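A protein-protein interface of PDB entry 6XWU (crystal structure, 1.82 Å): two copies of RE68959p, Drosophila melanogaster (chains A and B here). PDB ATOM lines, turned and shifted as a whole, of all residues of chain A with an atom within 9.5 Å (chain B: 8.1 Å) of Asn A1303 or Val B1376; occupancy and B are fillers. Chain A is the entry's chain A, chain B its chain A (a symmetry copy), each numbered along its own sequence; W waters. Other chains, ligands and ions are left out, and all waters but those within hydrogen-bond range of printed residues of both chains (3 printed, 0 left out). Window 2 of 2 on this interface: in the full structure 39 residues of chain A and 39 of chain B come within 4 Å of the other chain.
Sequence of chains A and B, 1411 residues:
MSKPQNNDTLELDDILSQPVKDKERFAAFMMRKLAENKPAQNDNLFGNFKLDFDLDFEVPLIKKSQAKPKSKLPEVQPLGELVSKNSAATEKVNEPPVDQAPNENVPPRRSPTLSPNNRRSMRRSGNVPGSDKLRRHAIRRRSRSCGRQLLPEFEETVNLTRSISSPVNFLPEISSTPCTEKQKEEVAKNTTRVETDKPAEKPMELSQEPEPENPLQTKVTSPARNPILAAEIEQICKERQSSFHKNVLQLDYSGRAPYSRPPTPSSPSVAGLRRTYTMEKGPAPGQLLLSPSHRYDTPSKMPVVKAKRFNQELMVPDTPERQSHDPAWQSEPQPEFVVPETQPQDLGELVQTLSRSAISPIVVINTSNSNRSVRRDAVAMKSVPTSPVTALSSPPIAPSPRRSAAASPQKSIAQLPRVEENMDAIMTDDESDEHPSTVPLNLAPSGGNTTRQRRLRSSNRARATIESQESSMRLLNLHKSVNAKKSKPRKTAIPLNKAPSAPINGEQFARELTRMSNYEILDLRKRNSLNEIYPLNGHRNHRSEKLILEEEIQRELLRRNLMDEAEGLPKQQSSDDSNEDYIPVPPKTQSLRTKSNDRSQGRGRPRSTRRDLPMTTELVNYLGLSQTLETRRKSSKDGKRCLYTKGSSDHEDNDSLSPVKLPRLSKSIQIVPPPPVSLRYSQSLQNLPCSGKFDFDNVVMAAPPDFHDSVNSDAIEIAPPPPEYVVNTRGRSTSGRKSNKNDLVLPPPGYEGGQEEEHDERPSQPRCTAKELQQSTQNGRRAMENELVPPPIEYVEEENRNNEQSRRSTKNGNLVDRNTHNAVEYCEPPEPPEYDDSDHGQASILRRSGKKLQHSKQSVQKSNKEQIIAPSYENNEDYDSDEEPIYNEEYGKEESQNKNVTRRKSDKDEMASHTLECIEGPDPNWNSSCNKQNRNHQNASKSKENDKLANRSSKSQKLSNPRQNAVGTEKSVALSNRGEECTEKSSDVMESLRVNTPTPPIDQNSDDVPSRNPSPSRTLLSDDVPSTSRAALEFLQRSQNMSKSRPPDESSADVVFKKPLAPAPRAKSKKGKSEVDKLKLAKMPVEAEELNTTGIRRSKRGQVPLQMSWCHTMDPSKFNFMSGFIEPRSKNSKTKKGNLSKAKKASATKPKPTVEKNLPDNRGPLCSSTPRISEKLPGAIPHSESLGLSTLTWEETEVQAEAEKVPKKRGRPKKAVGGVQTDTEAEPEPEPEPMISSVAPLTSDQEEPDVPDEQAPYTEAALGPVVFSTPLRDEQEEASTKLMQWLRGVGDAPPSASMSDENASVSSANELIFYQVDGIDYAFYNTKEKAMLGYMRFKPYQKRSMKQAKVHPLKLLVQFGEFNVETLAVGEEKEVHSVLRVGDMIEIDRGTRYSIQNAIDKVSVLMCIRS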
ATOM      1  N   SER A1298      13.556   1.103  15.658  1.00  0.00           N
ATOM      2  CA  SER A1298      13.878   0.668  14.312  1.00  0.00           C
ATOM      3  C   SER A1298      15.074  -0.270  14.345  1.00  0.00           C
ATOM      4  O   SER A1298      15.854  -0.289  15.304  1.00  0.00           O
ATOM      5  CB  SER A1298      14.161   1.874  13.402  1.00  0.00           C
ATOM      6  OG  SER A1298      15.045   1.533  12.354  1.00  0.00           O
ATOM      7  N   MET A1299      15.212  -1.053  13.274  1.00  0.00           N
ATOM      8  CA  MET A1299      16.420  -1.844  13.079  1.00  0.00           C
ATOM      9  C   MET A1299      17.620  -0.996  12.660  1.00  0.00           C
ATOM     10  O   MET A1299      18.715  -1.557  12.512  1.00  0.00           O
ATOM     11  CB  MET A1299      16.176  -2.936  12.028  1.00  0.00           C
ATOM     12  CG  MET A1299      14.998  -3.847  12.312  1.00  0.00           C
ATOM     13  SD  MET A1299      15.467  -5.342  13.202  1.00  0.00           S
ATOM     14  CE  MET A1299      16.344  -6.269  11.953  1.00  0.00           C
ATOM     15  N   SER A1300      17.458   0.324  12.465  1.00  0.00           N
ATOM     16  CA  SER A1300      18.600   1.145  12.058  1.00  0.00           C
ATOM     17  C   SER A1300      19.676   1.194  13.120  1.00  0.00           C
ATOM     18  O   SER A1300      20.797   1.623  12.830  1.00  0.00           O
ATOM     19  CB  SER A1300      18.176   2.578  11.724  1.00  0.00           C
ATOM     20  OG  SER A1300      17.124   2.586  10.787  1.00  0.00           O
ATOM     21  N   ASP A1301      19.371   0.770  14.340  1.00  0.00           N
ATOM     22  CA  ASP A1301      20.396   0.791  15.370  1.00  0.00           C
ATOM     23  C   ASP A1301      21.472  -0.245  15.113  1.00  0.00           C
ATOM     24  O   ASP A1301      22.554  -0.161  15.716  1.00  0.00           O
ATOM     25  CB  ASP A1301      19.766   0.605  16.765  1.00  0.00           C
ATOM     26  CG  ASP A1301      18.876  -0.639  16.872  1.00  0.00           C
ATOM     27  OD1 ASP A1301      19.032  -1.592  16.081  1.00  0.00           O
ATOM     28  OD2 ASP A1301      18.027  -0.667  17.786  1.00  0.00           O
ATOM     29  N   GLU A1302      21.192  -1.209  14.220  1.00  0.00           N
ATOM     30  CA  GLU A1302      22.144  -2.205  13.757  1.00  0.00           C
ATOM     31  C   GLU A1302      23.084  -1.686  12.685  1.00  0.00           C
ATOM     32  O   GLU A1302      24.074  -2.363  12.379  1.00  0.00           O
ATOM     33  CB  GLU A1302      21.408  -3.419  13.178  1.00  0.00           C
ATOM     34  CG  GLU A1302      20.522  -4.164  14.117  1.00  0.00           C
ATOM     35  CD  GLU A1302      20.208  -5.548  13.569  1.00  0.00           C
ATOM     36  OE1 GLU A1302      19.789  -5.661  12.392  1.00  0.00           O
ATOM     37  OE2 GLU A1302      20.436  -6.521  14.291  1.00  0.00           O
ATOM     38  N   ASN A1303      22.792  -0.539  12.080  1.00  0.00           N
ATOM     39  CA  ASN A1303      23.651  -0.043  11.015  1.00  0.00           C
ATOM     40  C   ASN A1303      25.007   0.355  11.573  1.00  0.00           C
ATOM     41  O   ASN A1303      25.096   0.936  12.654  1.00  0.00           O
ATOM     42  CB  ASN A1303      22.999   1.143  10.302  1.00  0.00           C
ATOM     43  CG  ASN A1303      21.856   0.699   9.403  1.00  0.00           C
ATOM     44  OD1 ASN A1303      21.717  -0.487   9.126  1.00  0.00           O
ATOM     45  ND2 ASN A1303      21.036   1.638   8.953  1.00  0.00           N
ATOM     46  N   ALA A1304      26.060   0.044  10.808  1.00  0.00           N
ATOM     47  CA  ALA A1304      27.433   0.329  11.219  1.00  0.00           C
ATOM     48  C   ALA A1304      27.601   1.764  11.702  1.00  0.00           C
ATOM     49  O   ALA A1304      28.212   2.017  12.747  1.00  0.00           O
ATOM     50  CB  ALA A1304      28.383   0.054  10.052  1.00  0.00           C
ATOM     51  N   SER A1305      27.084   2.721  10.945  1.00  0.00           N
ATOM     52  CA  SER A1305      27.354   4.114  11.235  1.00  0.00           C
ATOM     53  C   SER A1305      26.425   4.709  12.288  1.00  0.00           C
ATOM     54  O   SER A1305      26.625   5.861  12.671  1.00  0.00           O
ATOM     55  CB  SER A1305      27.270   4.931   9.946  1.00  0.00           C
ATOM     56  OG  SER A1305      28.183   4.419   8.992  1.00  0.00           O
ATOM     57  N   VAL A1306      25.431   3.962  12.773  1.00  0.00           N
ATOM     58  CA  VAL A1306      24.403   4.515  13.651  1.00  0.00           C
ATOM     59  C   VAL A1306      24.718   4.152  15.096  1.00  0.00           C
ATOM     60  O   VAL A1306      25.045   2.994  15.397  1.00  0.00           O
ATOM     61  CB  VAL A1306      22.999   4.017  13.263  1.00  0.00           C
ATOM     62  CG1 VAL A1306      21.980   4.450  14.320  1.00  0.00           C
ATOM     63  CG2 VAL A1306      22.608   4.553  11.896  1.00  0.00           C
ATOM     64  N   SER A1307      24.606   5.134  15.990  1.00  0.00           N
ATOM     65  CA  SER A1307      24.654   4.898  17.428  1.00  0.00           C
ATOM     66  C   SER A1307      23.361   5.432  18.039  1.00  0.00           C
ATOM     67  O   SER A1307      23.185   6.649  18.175  1.00  0.00           O
ATOM     68  CB  SER A1307      25.883   5.553  18.059  1.00  0.00           C
ATOM     69  OG  SER A1307      26.128   4.990  19.345  1.00  0.00           O
ATOM     70  N   SER A1308      22.456   4.530  18.403  1.00  0.00           N
ATOM     71  CA  SER A1308      21.175   5.011  18.900  1.00  0.00           C
ATOM     72  C   SER A1308      21.287   5.450  20.355  1.00  0.00           C
ATOM     73  O   SER A1308      22.203   5.059  21.089  1.00  0.00           O
ATOM     74  CB  SER A1308      20.099   3.933  18.757  1.00  0.00           C
ATOM     75  OG  SER A1308      20.156   3.015  19.823  1.00  0.00           O
ATOM     76  N   GLU A1311      21.808   2.863  22.882  1.00  0.00           N
ATOM     77  CA  GLU A1311      23.154   2.339  23.055  1.00  0.00           C
ATOM     78  C   GLU A1311      23.793   2.886  24.314  1.00  0.00           C
ATOM     79  O   GLU A1311      24.657   2.227  24.901  1.00  0.00           O
ATOM     80  CB  GLU A1311      24.033   2.688  21.850  1.00  0.00           C
ATOM     81  CG  GLU A1311      24.011   1.668  20.733  1.00  0.00           C
ATOM     82  CD  GLU A1311      25.347   1.534  20.036  1.00  0.00           C
ATOM     83  OE1 GLU A1311      25.623   2.330  19.122  1.00  0.00           O
ATOM     84  OE2 GLU A1311      26.125   0.627  20.402  1.00  0.00           O
ATOM     85  N   ASN A1326      28.904   4.866  20.775  1.00  0.00           N
ATOM     86  CA  ASN A1326      29.916   3.922  20.293  1.00  0.00           C
ATOM     87  C   ASN A1326      30.335   4.312  18.880  1.00  0.00           C
ATOM     88  O   ASN A1326      29.907   3.728  17.882  1.00  0.00           O
ATOM     89  CB  ASN A1326      29.391   2.495  20.349  1.00  0.00           C
ATOM     90  CG  ASN A1326      29.387   1.945  21.754  1.00  0.00           C
ATOM     91  OD1 ASN A1326      28.524   1.150  22.118  1.00  0.00           O
ATOM     92  ND2 ASN A1326      30.350   2.377  22.562  1.00  0.00           N
ATOM     93  N   ASN B1364      15.038  10.390   8.072  1.00  0.00           N
ATOM     94  CA  ASN B1364      15.539   9.284   7.268  1.00  0.00           C
ATOM     95  C   ASN B1364      16.831   9.759   6.617  1.00  0.00           C
ATOM     96  O   ASN B1364      16.869  10.852   6.041  1.00  0.00           O
ATOM     97  CB  ASN B1364      14.528   8.861   6.202  1.00  0.00           C
ATOM     98  CG  ASN B1364      13.176   8.490   6.792  1.00  0.00           C
ATOM     99  OD1 ASN B1364      13.096   7.887   7.866  1.00  0.00           O
ATOM    100  ND2 ASN B1364      12.104   8.853   6.093  1.00  0.00           N
ATOM    101  N   VAL B1365      17.903   8.982   6.767  1.00  0.00           N
ATOM    102  CA  VAL B1365      19.205   9.339   6.210  1.00  0.00           C
ATOM    103  C   VAL B1365      19.643   8.226   5.272  1.00  0.00           C
ATOM    104  O   VAL B1365      19.610   7.048   5.642  1.00  0.00           O
ATOM    105  CB  VAL B1365      20.270   9.567   7.301  1.00  0.00           C
ATOM    106  CG1 VAL B1365      21.580  10.056   6.665  1.00  0.00           C
ATOM    107  CG2 VAL B1365      19.791  10.587   8.355  1.00  0.00           C
ATOM    108  N   GLU B1366      20.054   8.600   4.069  1.00  0.00           N
ATOM    109  CA  GLU B1366      20.558   7.667   3.071  1.00  0.00           C
ATOM    110  C   GLU B1366      22.047   7.932   2.876  1.00  0.00           C
ATOM    111  O   GLU B1366      22.443   9.082   2.675  1.00  0.00           O
ATOM    112  CB  GLU B1366      19.773   7.840   1.772  1.00  0.00           C
ATOM    113  CG  GLU B1366      20.451   7.379   0.506  1.00  0.00           C
ATOM    114  CD  GLU B1366      19.766   7.943  -0.733  1.00  0.00           C
ATOM    115  OE1 GLU B1366      18.541   7.746  -0.874  1.00  0.00           O
ATOM    116  OE2 GLU B1366      20.452   8.577  -1.563  1.00  0.00           O
ATOM    117  N   THR B1367      22.873   6.883   2.964  1.00  0.00           N
ATOM    118  CA  THR B1367      24.322   7.044   2.859  1.00  0.00           C
ATOM    119  C   THR B1367      24.900   6.082   1.831  1.00  0.00           C
ATOM    120  O   THR B1367      24.400   4.970   1.638  1.00  0.00           O
ATOM    121  CB  THR B1367      25.050   6.800   4.207  1.00  0.00           C
ATOM    122  OG1 THR B1367      24.766   5.484   4.678  1.00  0.00           O
ATOM    123  CG2 THR B1367      24.619   7.811   5.271  1.00  0.00           C
ATOM    124  N   LEU B1368      25.985   6.515   1.195  1.00  0.00           N
ATOM    125  CA  LEU B1368      26.750   5.671   0.282  1.00  0.00           C
ATOM    126  C   LEU B1368      28.224   5.910   0.584  1.00  0.00           C
ATOM    127  O   LEU B1368      28.754   6.966   0.247  1.00  0.00           O
ATOM    128  CB  LEU B1368      26.418   6.000  -1.175  1.00  0.00           C
ATOM    129  CG  LEU B1368      27.141   5.233  -2.289  1.00  0.00           C
ATOM    130  CD1 LEU B1368      26.900   3.742  -2.126  1.00  0.00           C
ATOM    131  CD2 LEU B1368      26.694   5.709  -3.668  1.00  0.00           C
ATOM    132  N   ALA B1369      28.881   4.951   1.232  1.00  0.00           N
ATOM    133  CA  ALA B1369      30.274   5.149   1.619  1.00  0.00           C
ATOM    134  C   ALA B1369      31.226   4.878   0.448  1.00  0.00           C
ATOM    135  O   ALA B1369      30.886   4.197  -0.522  1.00  0.00           O
ATOM    136  CB  ALA B1369      30.634   4.255   2.808  1.00  0.00           C
ATOM    137  N   GLU B1372      31.850   1.289  -1.439  1.00  0.00           N
ATOM    138  CA  GLU B1372      30.614   0.532  -1.523  1.00  0.00           C
ATOM    139  C   GLU B1372      29.822   0.952  -2.757  1.00  0.00           C
ATOM    140  O   GLU B1372      29.991   2.049  -3.297  1.00  0.00           O
ATOM    141  CB  GLU B1372      29.775   0.737  -0.263  1.00  0.00           C
ATOM    142  CG  GLU B1372      30.596   0.824   1.010  1.00  0.00           C
ATOM    143  CD  GLU B1372      29.875   0.258   2.218  1.00  0.00           C
ATOM    144  OE1 GLU B1372      28.626   0.325   2.258  1.00  0.00           O
ATOM    145  OE2 GLU B1372      30.562  -0.245   3.132  1.00  0.00           O
ATOM    146  N   GLU B1373      28.948   0.058  -3.208  1.00  0.00           N
ATOM    147  CA  GLU B1373      28.054   0.359  -4.315  1.00  0.00           C
ATOM    148  C   GLU B1373      26.585   0.301  -3.917  1.00  0.00           C
ATOM    149  O   GLU B1373      25.719   0.597  -4.749  1.00  0.00           O
ATOM    150  CB  GLU B1373      28.311  -0.597  -5.489  1.00  0.00           C
ATOM    151  N   LYS B1374      26.278  -0.061  -2.674  1.00  0.00           N
ATOM    152  CA  LYS B1374      24.909  -0.184  -2.194  1.00  0.00           C
ATOM    153  C   LYS B1374      24.648   0.846  -1.105  1.00  0.00           C
ATOM    154  O   LYS B1374      25.394   0.918  -0.120  1.00  0.00           O
ATOM    155  CB  LYS B1374      24.646  -1.592  -1.660  1.00  0.00           C
ATOM    156  CG  LYS B1374      23.181  -1.941  -1.517  1.00  0.00           C
ATOM    157  CD  LYS B1374      23.010  -3.358  -0.989  1.00  0.00           C
ATOM    158  CE  LYS B1374      21.649  -3.531  -0.347  1.00  0.00           C
ATOM    159  NZ  LYS B1374      21.684  -4.528   0.756  1.00  0.00           N
ATOM    160  N   GLU B1375      23.583   1.625  -1.273  1.00  0.00           N
ATOM    161  CA  GLU B1375      23.201   2.603  -0.264  1.00  0.00           C
ATOM    162  C   GLU B1375      22.705   1.907   0.998  1.00  0.00           C
ATOM    163  O   GLU B1375      22.297   0.739   0.986  1.00  0.00           O
ATOM    164  CB  GLU B1375      22.097   3.525  -0.783  1.00  0.00           C
ATOM    165  CG  GLU B1375      22.494   4.465  -1.899  1.00  0.00           C
ATOM    166  CD  GLU B1375      21.283   4.994  -2.630  1.00  0.00           C
ATOM    167  OE1 GLU B1375      20.300   5.361  -1.955  1.00  0.00           O
ATOM    168  OE2 GLU B1375      21.321   5.054  -3.875  1.00  0.00           O
ATOM    169  N   VAL B1376      22.735   2.658   2.097  1.00  0.00           N
ATOM    170  CA  VAL B1376      22.196   2.243   3.390  1.00  0.00           C
ATOM    171  C   VAL B1376      21.182   3.291   3.822  1.00  0.00           C
ATOM    172  O   VAL B1376      21.484   4.488   3.804  1.00  0.00           O
ATOM    173  CB  VAL B1376      23.313   2.102   4.444  1.00  0.00           C
ATOM    174  CG1 VAL B1376      22.734   1.819   5.840  1.00  0.00           C
ATOM    175  CG2 VAL B1376      24.306   1.023   4.040  1.00  0.00           C
ATOM    176  N   HIS B1377      19.988   2.852   4.209  1.00  0.00           N
ATOM    177  CA  HIS B1377      18.970   3.753   4.737  1.00  0.00           C
ATOM    178  C   HIS B1377      18.850   3.563   6.240  1.00  0.00           C
ATOM    179  O   HIS B1377      18.747   2.429   6.714  1.00  0.00           O
ATOM    180  CB  HIS B1377      17.622   3.514   4.052  1.00  0.00           C
ATOM    181  CG  HIS B1377      17.595   3.955   2.623  1.00  0.00           C
ATOM    182  ND1 HIS B1377      18.096   3.185   1.595  1.00  0.00           N
ATOM    183  CD2 HIS B1377      17.149   5.099   2.054  1.00  0.00           C
ATOM    184  CE1 HIS B1377      17.948   3.831   0.451  1.00  0.00           C
ATOM    185  NE2 HIS B1377      17.376   4.995   0.703  1.00  0.00           N
ATOM    186  N   SER B1378      18.873   4.673   6.986  1.00  0.00           N
ATOM    187  CA  SER B1378      18.740   4.656   8.439  1.00  0.00           C
ATOM    188  C   SER B1378      17.603   5.586   8.851  1.00  0.00           C
ATOM    189  O   SER B1378      17.358   6.603   8.199  1.00  0.00           O
ATOM    190  CB  SER B1378      20.053   5.123   9.114  1.00  0.00           C
ATOM    191  OG  SER B1378      21.148   4.304   8.725  1.00  0.00           O
ATOM    192  N   VAL B1379      16.901   5.228   9.927  1.00  0.00           N
ATOM    193  CA  VAL B1379      15.905   6.097  10.553  1.00  0.00           C
ATOM    194  C   VAL B1379      16.427   6.501  11.926  1.00  0.00           C
ATOM    195  O   VAL B1379      16.880   5.644  12.699  1.00  0.00           O
ATOM    196  CB  VAL B1379      14.532   5.412  10.661  1.00  0.00           C
ATOM    197  CG1 VAL B1379      13.490   6.394  11.205  1.00  0.00           C
ATOM    198  CG2 VAL B1379      14.106   4.904   9.318  1.00  0.00           C
ATOM    199  N   LEU B1380      16.361   7.798  12.231  1.00  0.00           N
ATOM    200  CA  LEU B1380      16.937   8.368  13.445  1.00  0.00           C
ATOM    201  C   LEU B1380      15.871   9.134  14.214  1.00  0.00           C
ATOM    202  O   LEU B1380      15.210  10.010  13.649  1.00  0.00           O
ATOM    203  CB  LEU B1380      18.094   9.325  13.122  1.00  0.00           C
ATOM    204  CG  LEU B1380      19.320   8.815  12.361  1.00  0.00           C
ATOM    205  CD1 LEU B1380      20.330   9.956  12.160  1.00  0.00           C
ATOM    206  CD2 LEU B1380      19.958   7.632  13.104  1.00  0.00           C
ATOM    207  N   MET B1385      22.368   9.150  16.764  1.00  0.00           N
ATOM    208  CA  MET B1385      23.436   9.801  16.021  1.00  0.00           C
ATOM    209  C   MET B1385      23.869   8.910  14.857  1.00  0.00           C
ATOM    210  O   MET B1385      23.795   7.682  14.942  1.00  0.00           O
ATOM    211  CB  MET B1385      24.630  10.078  16.952  1.00  0.00           C
ATOM    212  CG  MET B1385      25.750  10.849  16.307  1.00  0.00           C
ATOM    213  SD  MET B1385      27.054   9.700  15.861  1.00  0.00           S
ATOM    214  CE  MET B1385      27.538   9.267  17.493  1.00  0.00           C
ATOM    215  N   ILE B1386      24.297   9.527  13.761  1.00  0.00           N
ATOM    216  CA  ILE B1386      24.920   8.787  12.664  1.00  0.00           C
ATOM    217  C   ILE B1386      26.242   9.464  12.332  1.00  0.00           C
ATOM    218  O   ILE B1386      26.346  10.699  12.338  1.00  0.00           O
ATOM    219  CB  ILE B1386      24.000   8.679  11.420  1.00  0.00           C
ATOM    220  CG1 ILE B1386      24.614   7.760  10.351  1.00  0.00           C
ATOM    221  CG2 ILE B1386      23.692  10.065  10.814  1.00  0.00           C
ATOM    222  CD1 ILE B1386      23.620   7.308   9.272  1.00  0.00           C
ATOM    223  N   GLU B1387      27.255   8.647  12.062  1.00  0.00           N
ATOM    224  CA  GLU B1387      28.590   9.103  11.698  1.00  0.00           C
ATOM    225  C   GLU B1387      28.725   9.022  10.184  1.00  0.00           C
ATOM    226  O   GLU B1387      28.454   7.970   9.595  1.00  0.00           O
ATOM    227  CB  GLU B1387      29.639   8.217  12.374  1.00  0.00           C
ATOM    228  CG  GLU B1387      30.989   8.848  12.653  1.00  0.00           C
ATOM    229  CD  GLU B1387      31.854   7.979  13.570  1.00  0.00           C
ATOM    230  OE1 GLU B1387      31.454   6.834  13.882  1.00  0.00           O
ATOM    231  OE2 GLU B1387      32.933   8.442  13.985  1.00  0.00           O
ATOM    232  N   ARG B1393      28.718   9.998   0.631  1.00  0.00           N
ATOM    233  CA  ARG B1393      27.633  10.833   0.115  1.00  0.00           C
ATOM    234  C   ARG B1393      26.371  10.553   0.917  1.00  0.00           C
ATOM    235  O   ARG B1393      26.081   9.401   1.249  1.00  0.00           O
ATOM    236  CB  ARG B1393      27.388  10.563  -1.374  1.00  0.00           C
ATOM    237  CG  ARG B1393      28.547  10.944  -2.282  1.00  0.00           C
ATOM    238  CD  ARG B1393      28.415  10.225  -3.634  1.00  0.00           C
ATOM    239  NE  ARG B1393      29.675   9.661  -4.114  1.00  0.00           N
ATOM    240  CZ  ARG B1393      30.277   8.598  -3.586  1.00  0.00           C
ATOM    241  NH1 ARG B1393      29.741   7.968  -2.548  1.00  0.00           N
ATOM    242  NH2 ARG B1393      31.423   8.161  -4.096  1.00  0.00           N
ATOM    243  N   TYR B1394      25.630  11.605   1.263  1.00  0.00           N
ATOM    244  CA  TYR B1394      24.495  11.391   2.152  1.00  0.00           C
ATOM    245  C   TYR B1394      23.374  12.372   1.843  1.00  0.00           C
ATOM    246  O   TYR B1394      23.624  13.523   1.473  1.00  0.00           O
ATOM    247  CB  TYR B1394      24.928  11.510   3.617  1.00  0.00           C
ATOM    248  CG  TYR B1394      25.297  12.922   4.043  1.00  0.00           C
ATOM    249  CD1 TYR B1394      26.520  13.479   3.682  1.00  0.00           C
ATOM    250  CD2 TYR B1394      24.429  13.689   4.820  1.00  0.00           C
ATOM    251  CE1 TYR B1394      26.863  14.761   4.063  1.00  0.00           C
ATOM    252  CE2 TYR B1394      24.764  14.980   5.206  1.00  0.00           C
ATOM    253  CZ  TYR B1394      25.986  15.511   4.818  1.00  0.00           C
ATOM    254  OH  TYR B1394      26.333  16.787   5.191  1.00  0.00           O
ATOM    255  N   SER B1395      22.134  11.900   2.014  1.00  0.00           N
ATOM    256  CA  SER B1395      20.927  12.698   1.856  1.00  0.00           C
ATOM    257  C   SER B1395      20.107  12.584   3.135  1.00  0.00           C
ATOM    258  O   SER B1395      20.160  11.561   3.822  1.00  0.00           O
ATOM    259  CB  SER B1395      20.090  12.218   0.654  1.00  0.00           C
ATOM    260  OG  SER B1395      20.691  12.589  -0.575  1.00  0.00           O
HETATM  261  O   HOH W   1      25.378   4.619   7.076  1.00  0.00           O
HETATM  262  O   HOH W   2      28.295   6.057  15.032  1.00  0.00           O
HETATM  263  O   HOH W   3      27.619   6.823   7.235  1.00  0.00           O
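Printed residues of chain B within 4 Å of Ser A1300: Ser B1378 and Val B1379. No residue of chain B comes within 4 Å of Ala A1304. Of the printed residues of chain B, Val A1306 touches Ser B1378 (3.5 Å), Leu B1380 (3.96 Å), Met B1385 (3.5 Å) and Ile B1386 (3.9 Å). Of the printed residues of chain B, Ser A1307 touches Met B1385 (2.9 Å). No residue of chain A comes within 4 Å of Thr B1367. Val B1376 touches just one residue of chain A: Asn A1303. Of chain A, only Asn A1303 (3.3 Å) comes within 4 Å of His B1377. Of the printed residues of chain A, Leu B1380 touches Val A1306 (3.96 Å). Of the printed residues of chain A, Glu B1387 touches Ser A1305 (2.9 Å).
O of His B1377 sits at hydrogen-bond distance from ND2 of Asn A1303 (3.3 Å). The side-chain hydroxyl (OG) of Ser A1300 is in hydrogen-bond range of the backbone NH (N) of Val B1379, 2.8 Å away. The side-chain hydroxyl of Ser B1378 is in hydrogen-bond range of the side-chain amide nitrogen of Asn A1303, at 2.7 Å. The backbone NH (N) of Glu B1387 sits at hydrogen-bond distance from the backbone carbonyl oxygen (O) of Ser A1305 (2.9 Å). The backbone NH of Ser A1307 lies within hydrogen-bond range of the backbone carbonyl oxygen of Met B1385 (2.9 Å).
The side-chain hydroxyl (OG) of Ser A1307 sits at hydrogen-bond distance from the backbone NH (N) of Asn A1326 (3.1 Å). OG of Ser A1298 is in hydrogen-bond range of N of Ser A1300 (2.7 Å). The side-chain carboxylate (OE1) of Glu B1366 is in hydrogen-bond range of a ring nitrogen (NE2) of His B1377 (3.4 Å). O of Thr B1367 lies within hydrogen-bond range of N of Val B1376 (2.9 Å). The backbone carbonyl oxygen (O) of Val B1365 is in hydrogen-bond range of the backbone NH (N) of Ser B1378, at 2.8 Å. The side-chain hydroxyl (OG) of Ser A1307 sits at hydrogen-bond distance from the side-chain carboxylate (OE1) of Glu A1311 (2.7 Å).
Water W1 bridges the side-chain hydroxyl of Thr B1367 (2.6 Å) and the side-chain hydroxyl of Ser A1305 (3.4 Å). Water W3 bridges the backbone carbonyl oxygen of Glu B1387 (2.8 Å) and the side-chain hydroxyl of Ser A1305 (3.0 Å). Water W2 lies within hydrogen-bond range of O of Ser A1305 (2.9 Å) and OE1 of Glu B1387 (3.5 Å).
Ser B1378 touches Ser A1300. ND2 of Asn A1303 touches CG1 of Val B1376 (3.6 Å). Ile B1386 touches Ser A1305 (CA to O, 3.4 Å). Ser B1378 touches Val A1306. Leu B1380 touches Val A1306. O of Met B1385 touches CA of Val A1306 (3.5 Å). CG2 of Val A1306 touches CD1 of Ile B1386, at 3.9 Å.
Hydrophobic or aromatic side chains of chain B that line the printed part of chain A: Val B1376, Val B1379, Leu B1380, Met B1385 and Ile B1386. Hydrophobic or aromatic side chains of chain A that line the printed part of chain B: Val A1306. Among the printed residues, no Asp or Glu carboxylate lies within 4 Å of a Lys or Arg side-chain nitrogen of the other chain.
No position is printed for both chains. Of the 12 pairs that touch across the chains among the printed residues, none has its exchanged pair printed and touching as well.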
